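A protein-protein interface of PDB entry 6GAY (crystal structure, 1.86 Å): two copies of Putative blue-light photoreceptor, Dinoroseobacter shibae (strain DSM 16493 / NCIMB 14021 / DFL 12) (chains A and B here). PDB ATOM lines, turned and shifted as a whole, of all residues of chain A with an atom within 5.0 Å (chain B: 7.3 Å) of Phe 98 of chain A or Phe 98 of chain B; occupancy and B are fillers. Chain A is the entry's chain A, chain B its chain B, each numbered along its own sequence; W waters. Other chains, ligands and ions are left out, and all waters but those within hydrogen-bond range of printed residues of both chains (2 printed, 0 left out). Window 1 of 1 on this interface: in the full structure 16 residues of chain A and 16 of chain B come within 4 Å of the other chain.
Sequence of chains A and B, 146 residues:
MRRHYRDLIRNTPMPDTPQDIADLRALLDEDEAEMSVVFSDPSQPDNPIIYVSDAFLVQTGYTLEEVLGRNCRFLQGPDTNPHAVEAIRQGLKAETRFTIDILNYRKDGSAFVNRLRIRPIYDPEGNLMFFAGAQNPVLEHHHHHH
O of Arg 97 of chain A sits at hydrogen-bond distance from N of Asp 101 of chain B (3.1 Å).
O of Thr 99 of chain A is in hydrogen-bond range of N of Thr 99 of chain B, 2.8 Å away.
O of Asp 101 of chain B sits at hydrogen-bond distance from OG1 of Thr 96 of chain A, 2.9 Å away.
The backbone carbonyl oxygen of Ile 100 of chain A lies within hydrogen-bond range of the backbone NH of Leu 116 of chain A.
O of Phe 98 of chain A lies within hydrogen-bond range of N of Ile 118 of chain A (2.8 Å).
The side-chain carboxylate (OE2) of Glu 86 of chain B lies within hydrogen-bond range of the side-chain amide nitrogen (NE2) of Gln 90 of chain B.
The backbone carbonyl oxygen (O) of Phe 98 of chain B lies within hydrogen-bond range of the backbone NH (N) of Ile 118 of chain B, 2.8 Å away.
The backbone carbonyl oxygen of Ile 100 of chain B is in hydrogen-bond range of the backbone NH of Leu 116 of chain B (2.9 Å).
O of Ala 87 of chain B touches CB of Ala 87 of chain A, at 3.5 Å.
N of Ala 87 of chain A touches CB of Gln 90 of chain B, at 3.8 Å.
Ala 87 of chain A touches Gly 91 of chain B (CB to N, 3.8 Å).
Phe 98 of chain A touches Phe 98 of chain B (CD2 to CE1, 3.7 Å).
CB of Phe 98 of chain A touches CG1 of Ile 100 of chain B, at 3.9 Å.
Thr 99 of chain A touches Arg 97 of chain B.
Phe 98 of chain B touches Thr 99 of chain A (CD1 to O, 3.2 Å).
CG1 of Ile 100 of chain A touches CG2 of Thr 96 of chain B, at 3.7 Å.
Arg 97 of chain B touches Ile 100 of chain A.
Phe 98 of chain B touches Ile 100 of chain A (CD1 to CD1, 3.6 Å).
Of the printed residues of chain B, Phe 98 of chain A touches Phe 98, Thr 99 and Ile 100.
Printed residues of chain B within 4 Å of Thr 99 of chain A: Arg 97, Phe 98 and Thr 99.
Arg 117 of chain A touches none of the printed residues of chain B.
Printed residues of chain A within 4 Å of Gln 90 of chain B: Ala 87 (3.8 Å).
Of the printed residues of chain A, Phe 98 of chain B touches Phe 98 (3.7 Å), Thr 99 (3.2 Å) and Ile 100 (3.6 Å).
The nearest printed residue of chain B that does not touch Phe 98 of chain A is Asp 101 of chain B (5.2 Å).
The nearest printed residue of chain A that does not touch Phe 98 of chain B is Ala 87 of chain A (4.02 Å).
Hydrophobic or aromatic side chains of chain B within 4 Å of the printed part of chain A: Ala 87, Phe 98 and Ile 100.
Along chain B the printed residues that touch a printed residue of chain A span positions 87 to 101.
Among the printed residues, 18 pairs touch across the chains.
Among the printed residues, no Asp or Glu carboxylate lies within 4 Å of a Lys or Arg side-chain nitrogen of the other chain.
Ala 87 of chain B touches its own counterpart, Ala 87 of chain A.
Arg 97 of chain A touches Ile 100 of chain B, and with the chains exchanged Ile 100 of chain A touches Arg 97 of chain B.
Phe 98 of chain A touches its own counterpart, Phe 98 of chain B.
Phe 98 of chain A touches Thr 99 of chain B, and with the chains exchanged Thr 99 of chain A touches Phe 98 of chain B.
Positions printed for both chains: 87, 88, 91, 92, 96, 97, 98, 99, 100, 116, 117 and 118.
Water W2 bridges the side-chain carboxylate of Asp 101 of chain B and the backbone carbonyl oxygen of Arg 97 of chain A.
Water W1 lies within hydrogen-bond range of the side-chain carboxylate of Asp 101 of chain B (3.0 Å), the backbone NH of Arg 97 of chain A (3.0 Å) and the side-chain hydroxyl of Thr 96 of chain A (3.3 Å).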
ATOM      1  N   ALA A  87      -2.420 -13.444   4.562  1.00  0.00           N
ATOM      2  CA  ALA A  87      -2.025 -12.698   5.759  1.00  0.00           C
ATOM      3  C   ALA A  87      -1.837 -13.650   6.937  1.00  0.00           C
ATOM      4  O   ALA A  87      -0.921 -13.490   7.743  1.00  0.00           O
ATOM      5  CB  ALA A  87      -3.049 -11.598   6.116  1.00  0.00           C
ATOM      6  N   ILE A  88      -2.713 -14.650   7.065  1.00  0.00           N
ATOM      7  CA  ILE A  88      -2.540 -15.661   8.124  1.00  0.00           C
ATOM      8  C   ILE A  88      -1.246 -16.434   7.951  1.00  0.00           C
ATOM      9  O   ILE A  88      -0.504 -16.685   8.918  1.00  0.00           O
ATOM     10  CB  ILE A  88      -3.722 -16.648   8.126  1.00  0.00           C
ATOM     11  CG1 ILE A  88      -5.063 -15.920   8.395  1.00  0.00           C
ATOM     12  CG2 ILE A  88      -3.449 -17.756   9.180  1.00  0.00           C
ATOM     13  CD1 ILE A  88      -6.297 -16.835   8.025  1.00  0.00           C
ATOM     14  N   GLY A  91       1.432 -14.223   9.131  1.00  0.00           N
ATOM     15  CA  GLY A  91       1.387 -14.039  10.571  1.00  0.00           C
ATOM     16  C   GLY A  91       1.944 -15.241  11.304  1.00  0.00           C
ATOM     17  O   GLY A  91       2.704 -15.093  12.268  1.00  0.00           O
ATOM     18  N   LEU A  92       1.609 -16.455  10.825  1.00  0.00           N
ATOM     19  CA  LEU A  92       2.170 -17.680  11.414  1.00  0.00           C
ATOM     20  C   LEU A  92       3.678 -17.718  11.218  1.00  0.00           C
ATOM     21  O   LEU A  92       4.401 -18.079  12.150  1.00  0.00           O
ATOM     22  CB  LEU A  92       1.548 -18.944  10.809  1.00  0.00           C
ATOM     23  CG  LEU A  92       0.076 -19.160  11.176  1.00  0.00           C
ATOM     24  CD1 LEU A  92      -0.447 -20.356  10.369  1.00  0.00           C
ATOM     25  CD2 LEU A  92      -0.029 -19.538  12.645  1.00  0.00           C
ATOM     26  N   THR A  96       3.767 -14.659  15.866  1.00  0.00           N
ATOM     27  CA  THR A  96       3.340 -13.494  16.666  1.00  0.00           C
ATOM     28  C   THR A  96       1.818 -13.553  16.804  1.00  0.00           C
ATOM     29  O   THR A  96       1.144 -14.222  16.009  1.00  0.00           O
ATOM     30  CB  THR A  96       3.778 -12.182  15.992  1.00  0.00           C
ATOM     31  OG1 THR A  96       3.668 -11.070  16.898  1.00  0.00           O
ATOM     32  CG2 THR A  96       2.919 -11.887  14.724  1.00  0.00           C
ATOM     33  N   ARG A  97       1.290 -12.839  17.796  1.00  0.00           N
ATOM     34  CA  ARG A  97      -0.168 -12.789  17.990  1.00  0.00           C
ATOM     35  C   ARG A  97      -0.779 -12.024  16.824  1.00  0.00           C
ATOM     36  O   ARG A  97      -0.325 -10.897  16.464  1.00  0.00           O
ATOM     37  CB  ARG A  97      -0.453 -12.052  19.292  1.00  0.00           C
ATOM     38  CG  ARG A  97      -1.965 -11.885  19.586  1.00  0.00           C
ATOM     39  CD  ARG A  97      -2.131 -10.924  20.797  1.00  0.00           C
ATOM     40  NE  ARG A  97      -3.552 -10.914  21.190  1.00  0.00           N
ATOM     41  CZ  ARG A  97      -4.465 -10.204  20.527  1.00  0.00           C
ATOM     42  NH1 ARG A  97      -4.092  -9.480  19.442  1.00  0.00           N
ATOM     43  NH2 ARG A  97      -5.721 -10.189  20.967  1.00  0.00           N
ATOM     44  N   PHE A  98      -1.776 -12.602  16.203  1.00  0.00           N
ATOM     45  CA  PHE A  98      -2.495 -11.776  15.251  1.00  0.00           C
ATOM     46  C   PHE A  98      -3.931 -12.239  15.069  1.00  0.00           C
ATOM     47  O   PHE A  98      -4.277 -13.384  15.352  1.00  0.00           O
ATOM     48  CB  PHE A  98      -1.811 -11.757  13.880  1.00  0.00           C
ATOM     49  CG  PHE A  98      -1.915 -13.010  13.190  1.00  0.00           C
ATOM     50  CD1 PHE A  98      -1.028 -14.063  13.531  1.00  0.00           C
ATOM     51  CD2 PHE A  98      -2.878 -13.194  12.194  1.00  0.00           C
ATOM     52  CE1 PHE A  98      -1.084 -15.332  12.856  1.00  0.00           C
ATOM     53  CE2 PHE A  98      -3.003 -14.441  11.570  1.00  0.00           C
ATOM     54  CZ  PHE A  98      -2.106 -15.506  11.885  1.00  0.00           C
ATOM     55  N   THR A  99      -4.732 -11.326  14.549  1.00  0.00           N
ATOM     56  CA  THR A  99      -6.176 -11.520  14.385  1.00  0.00           C
ATOM     57  C   THR A  99      -6.648 -11.035  13.019  1.00  0.00           C
ATOM     58  O   THR A  99      -6.217  -9.974  12.562  1.00  0.00           O
ATOM     59  CB  THR A  99      -6.931 -10.724  15.431  1.00  0.00           C
ATOM     60  OG1 THR A  99      -6.468 -11.067  16.715  1.00  0.00           O
ATOM     61  CG2 THR A  99      -8.481 -10.884  15.315  1.00  0.00           C
ATOM     62  N   ILE A 100      -7.535 -11.789  12.336  1.00  0.00           N
ATOM     63  CA  ILE A 100      -8.031 -11.338  11.045  1.00  0.00           C
ATOM     64  C   ILE A 100      -9.491 -11.762  10.922  1.00  0.00           C
ATOM     65  O   ILE A 100      -9.899 -12.816  11.437  1.00  0.00           O
ATOM     66  CB  ILE A 100      -7.207 -11.919   9.871  1.00  0.00           C
ATOM     67  CG1 ILE A 100      -7.597 -11.231   8.553  1.00  0.00           C
ATOM     68  CG2 ILE A 100      -7.440 -13.478   9.704  1.00  0.00           C
ATOM     69  CD1 ILE A 100      -6.439 -11.243   7.471  1.00  0.00           C
ATOM     70  N   LEU A 116     -10.756 -14.460  13.611  1.00  0.00           N
ATOM     71  CA  LEU A 116      -9.858 -15.544  14.028  1.00  0.00           C
ATOM     72  C   LEU A 116      -8.686 -14.945  14.788  1.00  0.00           C
ATOM     73  O   LEU A 116      -7.984 -14.068  14.244  1.00  0.00           O
ATOM     74  CB  LEU A 116      -9.334 -16.271  12.794  1.00  0.00           C
ATOM     75  CG  LEU A 116      -8.109 -17.180  12.957  1.00  0.00           C
ATOM     76  CD1 LEU A 116      -8.566 -18.384  13.811  1.00  0.00           C
ATOM     77  CD2 LEU A 116      -7.781 -17.617  11.530  1.00  0.00           C
ATOM     78  N   ARG A 117      -8.508 -15.370  16.029  1.00  0.00           N
ATOM     79  CA  ARG A 117      -7.450 -14.838  16.903  1.00  0.00           C
ATOM     80  C   ARG A 117      -6.415 -15.913  17.101  1.00  0.00           C
ATOM     81  O   ARG A 117      -6.681 -16.929  17.787  1.00  0.00           O
ATOM     82  CB  ARG A 117      -7.997 -14.401  18.260  1.00  0.00           C
ATOM     83  CG  ARG A 117      -8.897 -13.195  18.163  1.00  0.00           C
ATOM     84  CD  ARG A 117      -9.215 -12.647  19.496  1.00  0.00           C
ATOM     85  NE  ARG A 117      -9.735 -11.242  19.331  1.00  0.00           N
ATOM     86  CZ  ARG A 117     -11.039 -10.917  19.280  1.00  0.00           C
ATOM     87  NH1 ARG A 117     -12.004 -11.859  19.451  1.00  0.00           N
ATOM     88  NH2 ARG A 117     -11.385  -9.652  19.110  1.00  0.00           N
ATOM     89  N   ILE A 118      -5.206 -15.691  16.573  1.00  0.00           N
ATOM     90  CA  ILE A 118      -4.180 -16.728  16.683  1.00  0.00           C
ATOM     91  C   ILE A 118      -3.066 -16.209  17.594  1.00  0.00           C
ATOM     92  O   ILE A 118      -2.759 -14.997  17.581  1.00  0.00           O
ATOM     93  CB  ILE A 118      -3.670 -17.101  15.275  1.00  0.00           C
ATOM     94  CG1 ILE A 118      -4.633 -18.048  14.574  1.00  0.00           C
ATOM     95  CG2 ILE A 118      -2.222 -17.655  15.333  1.00  0.00           C
ATOM     96  CD1 ILE A 118      -4.380 -18.062  13.091  1.00  0.00           C
ATOM     97  N   HIS B  83       7.883 -11.004   7.859  1.00  0.00           N
ATOM     98  CA  HIS B  83       6.644 -11.724   7.645  1.00  0.00           C
ATOM     99  C   HIS B  83       5.464 -10.958   8.235  1.00  0.00           C
ATOM    100  O   HIS B  83       4.352 -10.987   7.667  1.00  0.00           O
ATOM    101  CB  HIS B  83       6.752 -13.155   8.258  1.00  0.00           C
ATOM    102  CG  HIS B  83       7.766 -14.023   7.567  1.00  0.00           C
ATOM    103  ND1 HIS B  83       7.545 -14.577   6.315  1.00  0.00           N
ATOM    104  CD2 HIS B  83       9.016 -14.422   7.939  1.00  0.00           C
ATOM    105  CE1 HIS B  83       8.605 -15.295   5.957  1.00  0.00           C
ATOM    106  NE2 HIS B  83       9.514 -15.205   6.914  1.00  0.00           N
ATOM    107  N   ALA B  84       5.662 -10.262   9.369  1.00  0.00           N
ATOM    108  CA  ALA B  84       4.565  -9.445   9.893  1.00  0.00           C
ATOM    109  C   ALA B  84       4.279  -8.279   8.961  1.00  0.00           C
ATOM    110  O   ALA B  84       3.118  -7.886   8.767  1.00  0.00           O
ATOM    111  CB  ALA B  84       4.907  -8.919  11.266  1.00  0.00           C
ATOM    112  N   VAL B  85       5.337  -7.684   8.401  1.00  0.00           N
ATOM    113  CA  VAL B  85       5.117  -6.628   7.408  1.00  0.00           C
ATOM    114  C   VAL B  85       4.249  -7.136   6.242  1.00  0.00           C
ATOM    115  O   VAL B  85       3.292  -6.476   5.844  1.00  0.00           O
ATOM    116  CB  VAL B  85       6.467  -6.077   6.914  1.00  0.00           C
ATOM    117  CG1 VAL B  85       6.262  -5.070   5.783  1.00  0.00           C
ATOM    118  CG2 VAL B  85       7.180  -5.413   8.096  1.00  0.00           C
ATOM    119  N   GLU B  86       4.566  -8.317   5.693  1.00  0.00           N
ATOM    120  CA  GLU B  86       3.810  -8.847   4.550  1.00  0.00           C
ATOM    121  C   GLU B  86       2.401  -9.213   4.975  1.00  0.00           C
ATOM    122  O   GLU B  86       1.431  -9.012   4.210  1.00  0.00           O
ATOM    123  CB  GLU B  86       4.527 -10.048   3.927  1.00  0.00           C
ATOM    124  CG  GLU B  86       3.827 -10.668   2.722  1.00  0.00           C
ATOM    125  CD  GLU B  86       3.608  -9.707   1.524  1.00  0.00           C
ATOM    126  OE1 GLU B  86       4.334  -8.686   1.405  1.00  0.00           O
ATOM    127  OE2 GLU B  86       2.703  -9.977   0.692  1.00  0.00           O
ATOM    128  N   ALA B  87       2.265  -9.645   6.230  1.00  0.00           N
ATOM    129  CA  ALA B  87       0.936  -9.937   6.753  1.00  0.00           C
ATOM    130  C   ALA B  87       0.090  -8.685   6.787  1.00  0.00           C
ATOM    131  O   ALA B  87      -1.082  -8.720   6.427  1.00  0.00           O
ATOM    132  CB  ALA B  87       1.028 -10.568   8.137  1.00  0.00           C
ATOM    133  N   ILE B  88       0.661  -7.553   7.216  1.00  0.00           N
ATOM    134  CA  ILE B  88      -0.107  -6.320   7.150  1.00  0.00           C
ATOM    135  C   ILE B  88      -0.460  -5.988   5.706  1.00  0.00           C
ATOM    136  O   ILE B  88      -1.631  -5.706   5.401  1.00  0.00           O
ATOM    137  CB  ILE B  88       0.668  -5.186   7.782  1.00  0.00           C
ATOM    138  CG1 ILE B  88       0.784  -5.497   9.224  1.00  0.00           C
ATOM    139  CG2 ILE B  88      -0.026  -3.847   7.459  1.00  0.00           C
ATOM    140  CD1 ILE B  88       1.968  -4.639   9.840  1.00  0.00           C
ATOM    141  N   ARG B  89       0.544  -6.047   4.783  1.00  0.00           N
ATOM    142  CA  ARG B  89       0.265  -5.733   3.388  1.00  0.00           C
ATOM    143  C   ARG B  89      -0.934  -6.542   2.873  1.00  0.00           C
ATOM    144  O   ARG B  89      -1.832  -6.022   2.171  1.00  0.00           O
ATOM    145  CB  ARG B  89       1.482  -6.007   2.516  1.00  0.00           C
ATOM    146  CG  ARG B  89       1.462  -5.180   1.252  1.00  0.00           C
ATOM    147  CD  ARG B  89       2.789  -5.207   0.500  1.00  0.00           C
ATOM    148  NE  ARG B  89       2.964  -6.506  -0.108  1.00  0.00           N
ATOM    149  CZ  ARG B  89       2.579  -6.818  -1.339  1.00  0.00           C
ATOM    150  NH1 ARG B  89       2.749  -8.060  -1.761  1.00  0.00           N
ATOM    151  NH2 ARG B  89       2.028  -5.896  -2.136  1.00  0.00           N
ATOM    152  N   GLN B  90      -0.928  -7.833   3.147  1.00  0.00           N
ATOM    153  CA  GLN B  90      -2.037  -8.689   2.664  1.00  0.00           C
ATOM    154  C   GLN B  90      -3.363  -8.359   3.332  1.00  0.00           C
ATOM    155  O   GLN B  90      -4.420  -8.405   2.675  1.00  0.00           O
ATOM    156  CB  GLN B  90      -1.672 -10.153   2.883  1.00  0.00           C
ATOM    157  CG  GLN B  90      -0.477 -10.499   1.952  1.00  0.00           C
ATOM    158  CD  GLN B  90      -0.873 -10.540   0.496  1.00  0.00           C
ATOM    159  OE1 GLN B  90      -2.023 -10.868   0.127  1.00  0.00           O
ATOM    160  NE2 GLN B  90       0.075 -10.203  -0.362  1.00  0.00           N
ATOM    161  N   GLY B  91      -3.349  -8.080   4.645  1.00  0.00           N
ATOM    162  CA  GLY B  91      -4.590  -7.705   5.313  1.00  0.00           C
ATOM    163  C   GLY B  91      -5.209  -6.471   4.705  1.00  0.00           C
ATOM    164  O   GLY B  91      -6.429  -6.393   4.542  1.00  0.00           O
ATOM    165  N   LEU B  92      -4.374  -5.471   4.349  1.00  0.00           N
ATOM    166  CA  LEU B  92      -4.902  -4.311   3.653  1.00  0.00           C
ATOM    167  C   LEU B  92      -5.507  -4.698   2.309  1.00  0.00           C
ATOM    168  O   LEU B  92      -6.557  -4.172   1.920  1.00  0.00           O
ATOM    169  CB  LEU B  92      -3.792  -3.245   3.470  1.00  0.00           C
ATOM    170  CG  LEU B  92      -3.231  -2.708   4.791  1.00  0.00           C
ATOM    171  CD1 LEU B  92      -2.075  -1.728   4.457  1.00  0.00           C
ATOM    172  CD2 LEU B  92      -4.302  -2.006   5.603  1.00  0.00           C
ATOM    173  N   GLU B  95      -8.866  -5.819   2.576  1.00  0.00           N
ATOM    174  CA  GLU B  95      -9.761  -4.778   3.121  1.00  0.00           C
ATOM    175  C   GLU B  95     -10.569  -5.342   4.276  1.00  0.00           C
ATOM    176  O   GLU B  95     -11.776  -5.341   4.251  1.00  0.00           O
ATOM    177  CB  GLU B  95     -10.732  -4.248   2.073  1.00  0.00           C
ATOM    178  CG  GLU B  95     -10.004  -3.538   0.966  1.00  0.00           C
ATOM    179  CD  GLU B  95     -10.912  -2.926  -0.112  1.00  0.00           C
ATOM    180  OE1 GLU B  95     -12.154  -2.839   0.072  1.00  0.00           O
ATOM    181  OE2 GLU B  95     -10.314  -2.527  -1.128  1.00  0.00           O
ATOM    182  N   THR B  96      -9.876  -5.849   5.264  1.00  0.00           N
ATOM    183  CA  THR B  96     -10.553  -6.508   6.354  1.00  0.00           C
ATOM    184  C   THR B  96      -9.908  -6.032   7.627  1.00  0.00           C
ATOM    185  O   THR B  96      -8.755  -5.580   7.626  1.00  0.00           O
ATOM    186  CB  THR B  96     -10.443  -8.039   6.213  1.00  0.00           C
ATOM    187  OG1 THR B  96     -11.400  -8.714   7.077  1.00  0.00           O
ATOM    188  CG2 THR B  96      -8.992  -8.508   6.547  1.00  0.00           C
ATOM    189  N   ARG B  97     -10.641  -6.139   8.731  1.00  0.00           N
ATOM    190  CA  ARG B  97     -10.055  -5.835  10.046  1.00  0.00           C
ATOM    191  C   ARG B  97      -8.913  -6.799  10.370  1.00  0.00           C
ATOM    192  O   ARG B  97      -9.061  -8.023  10.235  1.00  0.00           O
ATOM    193  CB  ARG B  97     -11.139  -5.932  11.130  1.00  0.00           C
ATOM    194  CG  ARG B  97     -10.600  -5.623  12.546  1.00  0.00           C
ATOM    195  CD  ARG B  97     -11.666  -6.016  13.553  1.00  0.00           C
ATOM    196  NE  ARG B  97     -11.305  -5.652  14.919  1.00  0.00           N
ATOM    197  CZ  ARG B  97     -10.486  -6.354  15.730  1.00  0.00           C
ATOM    198  NH1 ARG B  97      -9.941  -7.522  15.328  1.00  0.00           N
ATOM    199  NH2 ARG B  97     -10.235  -5.915  16.966  1.00  0.00           N
ATOM    200  N   PHE B  98      -7.779  -6.281  10.849  1.00  0.00           N
ATOM    201  CA  PHE B  98      -6.552  -7.072  11.068  1.00  0.00           C
ATOM    202  C   PHE B  98      -5.808  -6.512  12.279  1.00  0.00           C
ATOM    203  O   PHE B  98      -5.597  -5.278  12.291  1.00  0.00           O
ATOM    204  CB  PHE B  98      -5.579  -6.980   9.850  1.00  0.00           C
ATOM    205  CG  PHE B  98      -4.382  -7.943   9.916  1.00  0.00           C
ATOM    206  CD1 PHE B  98      -4.581  -9.338   9.851  1.00  0.00           C
ATOM    207  CD2 PHE B  98      -3.072  -7.487  10.067  1.00  0.00           C
ATOM    208  CE1 PHE B  98      -3.489 -10.340   9.909  1.00  0.00           C
ATOM    209  CE2 PHE B  98      -1.983  -8.475  10.137  1.00  0.00           C
ATOM    210  CZ  PHE B  98      -2.239  -9.893  10.067  1.00  0.00           C
ATOM    211  N   THR B  99      -5.257  -7.370  13.147  1.00  0.00           N
ATOM    212  CA  THR B  99      -4.433  -6.983  14.304  1.00  0.00           C
ATOM    213  C   THR B  99      -3.154  -7.783  14.261  1.00  0.00           C
ATOM    214  O   THR B  99      -3.196  -8.973  13.995  1.00  0.00           O
ATOM    215  CB  THR B  99      -5.129  -7.247  15.603  1.00  0.00           C
ATOM    216  OG1 THR B  99      -6.311  -6.423  15.608  1.00  0.00           O
ATOM    217  CG2 THR B  99      -4.215  -6.860  16.897  1.00  0.00           C
ATOM    218  N   ILE B 100      -1.992  -7.150  14.499  1.00  0.00           N
ATOM    219  CA  ILE B 100      -0.786  -7.955  14.604  1.00  0.00           C
ATOM    220  C   ILE B 100       0.178  -7.290  15.598  1.00  0.00           C
ATOM    221  O   ILE B 100       0.274  -6.057  15.666  1.00  0.00           O
ATOM    222  CB  ILE B 100      -0.100  -8.122  13.211  1.00  0.00           C
ATOM    223  CG1 ILE B 100       1.069  -9.138  13.287  1.00  0.00           C
ATOM    224  CG2 ILE B 100       0.326  -6.771  12.606  1.00  0.00           C
ATOM    225  CD1 ILE B 100       1.402  -9.721  11.894  1.00  0.00           C
ATOM    226  N   ASP B 101       0.975  -8.105  16.271  1.00  0.00           N
ATOM    227  CA  ASP B 101       2.028  -7.589  17.163  1.00  0.00           C
ATOM    228  C   ASP B 101       3.270  -7.451  16.307  1.00  0.00           C
ATOM    229  O   ASP B 101       3.781  -8.445  15.789  1.00  0.00           O
ATOM    230  CB  ASP B 101       2.282  -8.530  18.349  1.00  0.00           C
ATOM    231  CG  ASP B 101       1.286  -8.343  19.464  1.00  0.00           C
ATOM    232  OD1 ASP B 101       0.247  -7.660  19.204  1.00  0.00           O
ATOM    233  OD2 ASP B 101       1.505  -8.913  20.586  1.00  0.00           O
ATOM    234  N   LEU B 116      -0.850  -3.571  16.732  1.00  0.00           N
ATOM    235  CA  LEU B 116      -1.359  -2.687  15.696  1.00  0.00           C
ATOM    236  C   LEU B 116      -2.722  -3.207  15.267  1.00  0.00           C
ATOM    237  O   LEU B 116      -2.783  -4.315  14.781  1.00  0.00           O
ATOM    238  CB  LEU B 116      -0.447  -2.695  14.476  1.00  0.00           C
ATOM    239  CG  LEU B 116      -0.973  -1.957  13.206  1.00  0.00           C
ATOM    240  CD1 LEU B 116      -1.242  -0.455  13.466  1.00  0.00           C
ATOM    241  CD2 LEU B 116       0.096  -2.145  12.194  1.00  0.00           C
ATOM    242  N   ARG B 117      -3.764  -2.382  15.385  1.00  0.00           N
ATOM    243  CA  ARG B 117      -5.136  -2.740  15.024  1.00  0.00           C
ATOM    244  C   ARG B 117      -5.555  -1.874  13.851  1.00  0.00           C
ATOM    245  O   ARG B 117      -5.834  -0.680  14.012  1.00  0.00           O
ATOM    246  CB  ARG B 117      -6.090  -2.552  16.219  1.00  0.00           C
ATOM    247  CG  ARG B 117      -5.751  -3.506  17.376  1.00  0.00           C
ATOM    248  CD  ARG B 117      -6.971  -3.563  18.349  1.00  0.00           C
ATOM    249  NE  ARG B 117      -6.760  -4.630  19.335  1.00  0.00           N
ATOM    250  CZ  ARG B 117      -6.151  -4.471  20.484  1.00  0.00           C
ATOM    251  NH1 ARG B 117      -5.702  -3.257  20.849  1.00  0.00           N
ATOM    252  NH2 ARG B 117      -6.016  -5.516  21.280  1.00  0.00           N
ATOM    253  N   ILE B 118      -5.684  -2.493  12.677  1.00  0.00           N
ATOM    254  CA  ILE B 118      -6.164  -1.817  11.470  1.00  0.00           C
ATOM    255  C   ILE B 118      -7.614  -2.179  11.222  1.00  0.00           C
ATOM    256  O   ILE B 118      -7.986  -3.345  11.364  1.00  0.00           O
ATOM    257  CB  ILE B 118      -5.268  -2.214  10.299  1.00  0.00           C
ATOM    258  CG1 ILE B 118      -3.923  -1.457  10.522  1.00  0.00           C
ATOM    259  CG2 ILE B 118      -5.920  -1.830   8.977  1.00  0.00           C
ATOM    260  CD1 ILE B 118      -2.750  -2.078   9.736  1.00  0.00           C
ATOM    261  N   ARG B 119      -8.425  -1.206  10.760  1.00  0.00           N
ATOM    262  CA  ARG B 119      -9.781  -1.550  10.383  1.00  0.00           C
ATOM    263  C   ARG B 119     -10.149  -0.709   9.188  1.00  0.00           C
ATOM    264  O   ARG B 119      -9.689   0.430   9.083  1.00  0.00           O
ATOM    265  CB  ARG B 119     -10.771  -1.290  11.532  1.00  0.00           C
ATOM    266  CG  ARG B 119     -10.824   0.216  11.911  1.00  0.00           C
ATOM    267  CD  ARG B 119     -11.564   0.391  13.212  1.00  0.00           C
ATOM    268  NE  ARG B 119     -11.872   1.817  13.565  1.00  0.00           N
ATOM    269  CZ  ARG B 119     -11.057   2.615  14.272  1.00  0.00           C
ATOM    270  NH1 ARG B 119      -9.872   2.169  14.722  1.00  0.00           N
ATOM    271  NH2 ARG B 119     -11.445   3.869  14.560  1.00  0.00           N
ATOM    272  N   PRO B 120     -10.974  -1.229   8.278  1.00  0.00           N
ATOM    273  CA  PRO B 120     -11.486  -0.396   7.180  1.00  0.00           C
ATOM    274  C   PRO B 120     -12.605   0.519   7.636  1.00  0.00           C
ATOM    275  O   PRO B 120     -13.380   0.200   8.543  1.00  0.00           O
ATOM    276  CB  PRO B 120     -12.003  -1.430   6.168  1.00  0.00           C
ATOM    277  CG  PRO B 120     -12.514  -2.570   7.101  1.00  0.00           C
ATOM    278  CD  PRO B 120     -11.474  -2.632   8.182  1.00  0.00           C
ATOM    279  N   ALA B 132      -8.087   2.929   9.258  1.00  0.00           N
ATOM    280  CA  ALA B 132      -7.737   3.457  10.565  1.00  0.00           C
ATOM    281  C   ALA B 132      -6.781   2.445  11.178  1.00  0.00           C
ATOM    282  O   ALA B 132      -7.001   1.234  11.066  1.00  0.00           O
ATOM    283  CB  ALA B 132      -8.964   3.634  11.460  1.00  0.00           C
HETATM  284  O   HOH W   1       2.851 -11.521  20.025  1.00  0.00           O
HETATM  285  O   HOH W   2      -1.653  -8.926  17.973  1.00  0.00           O
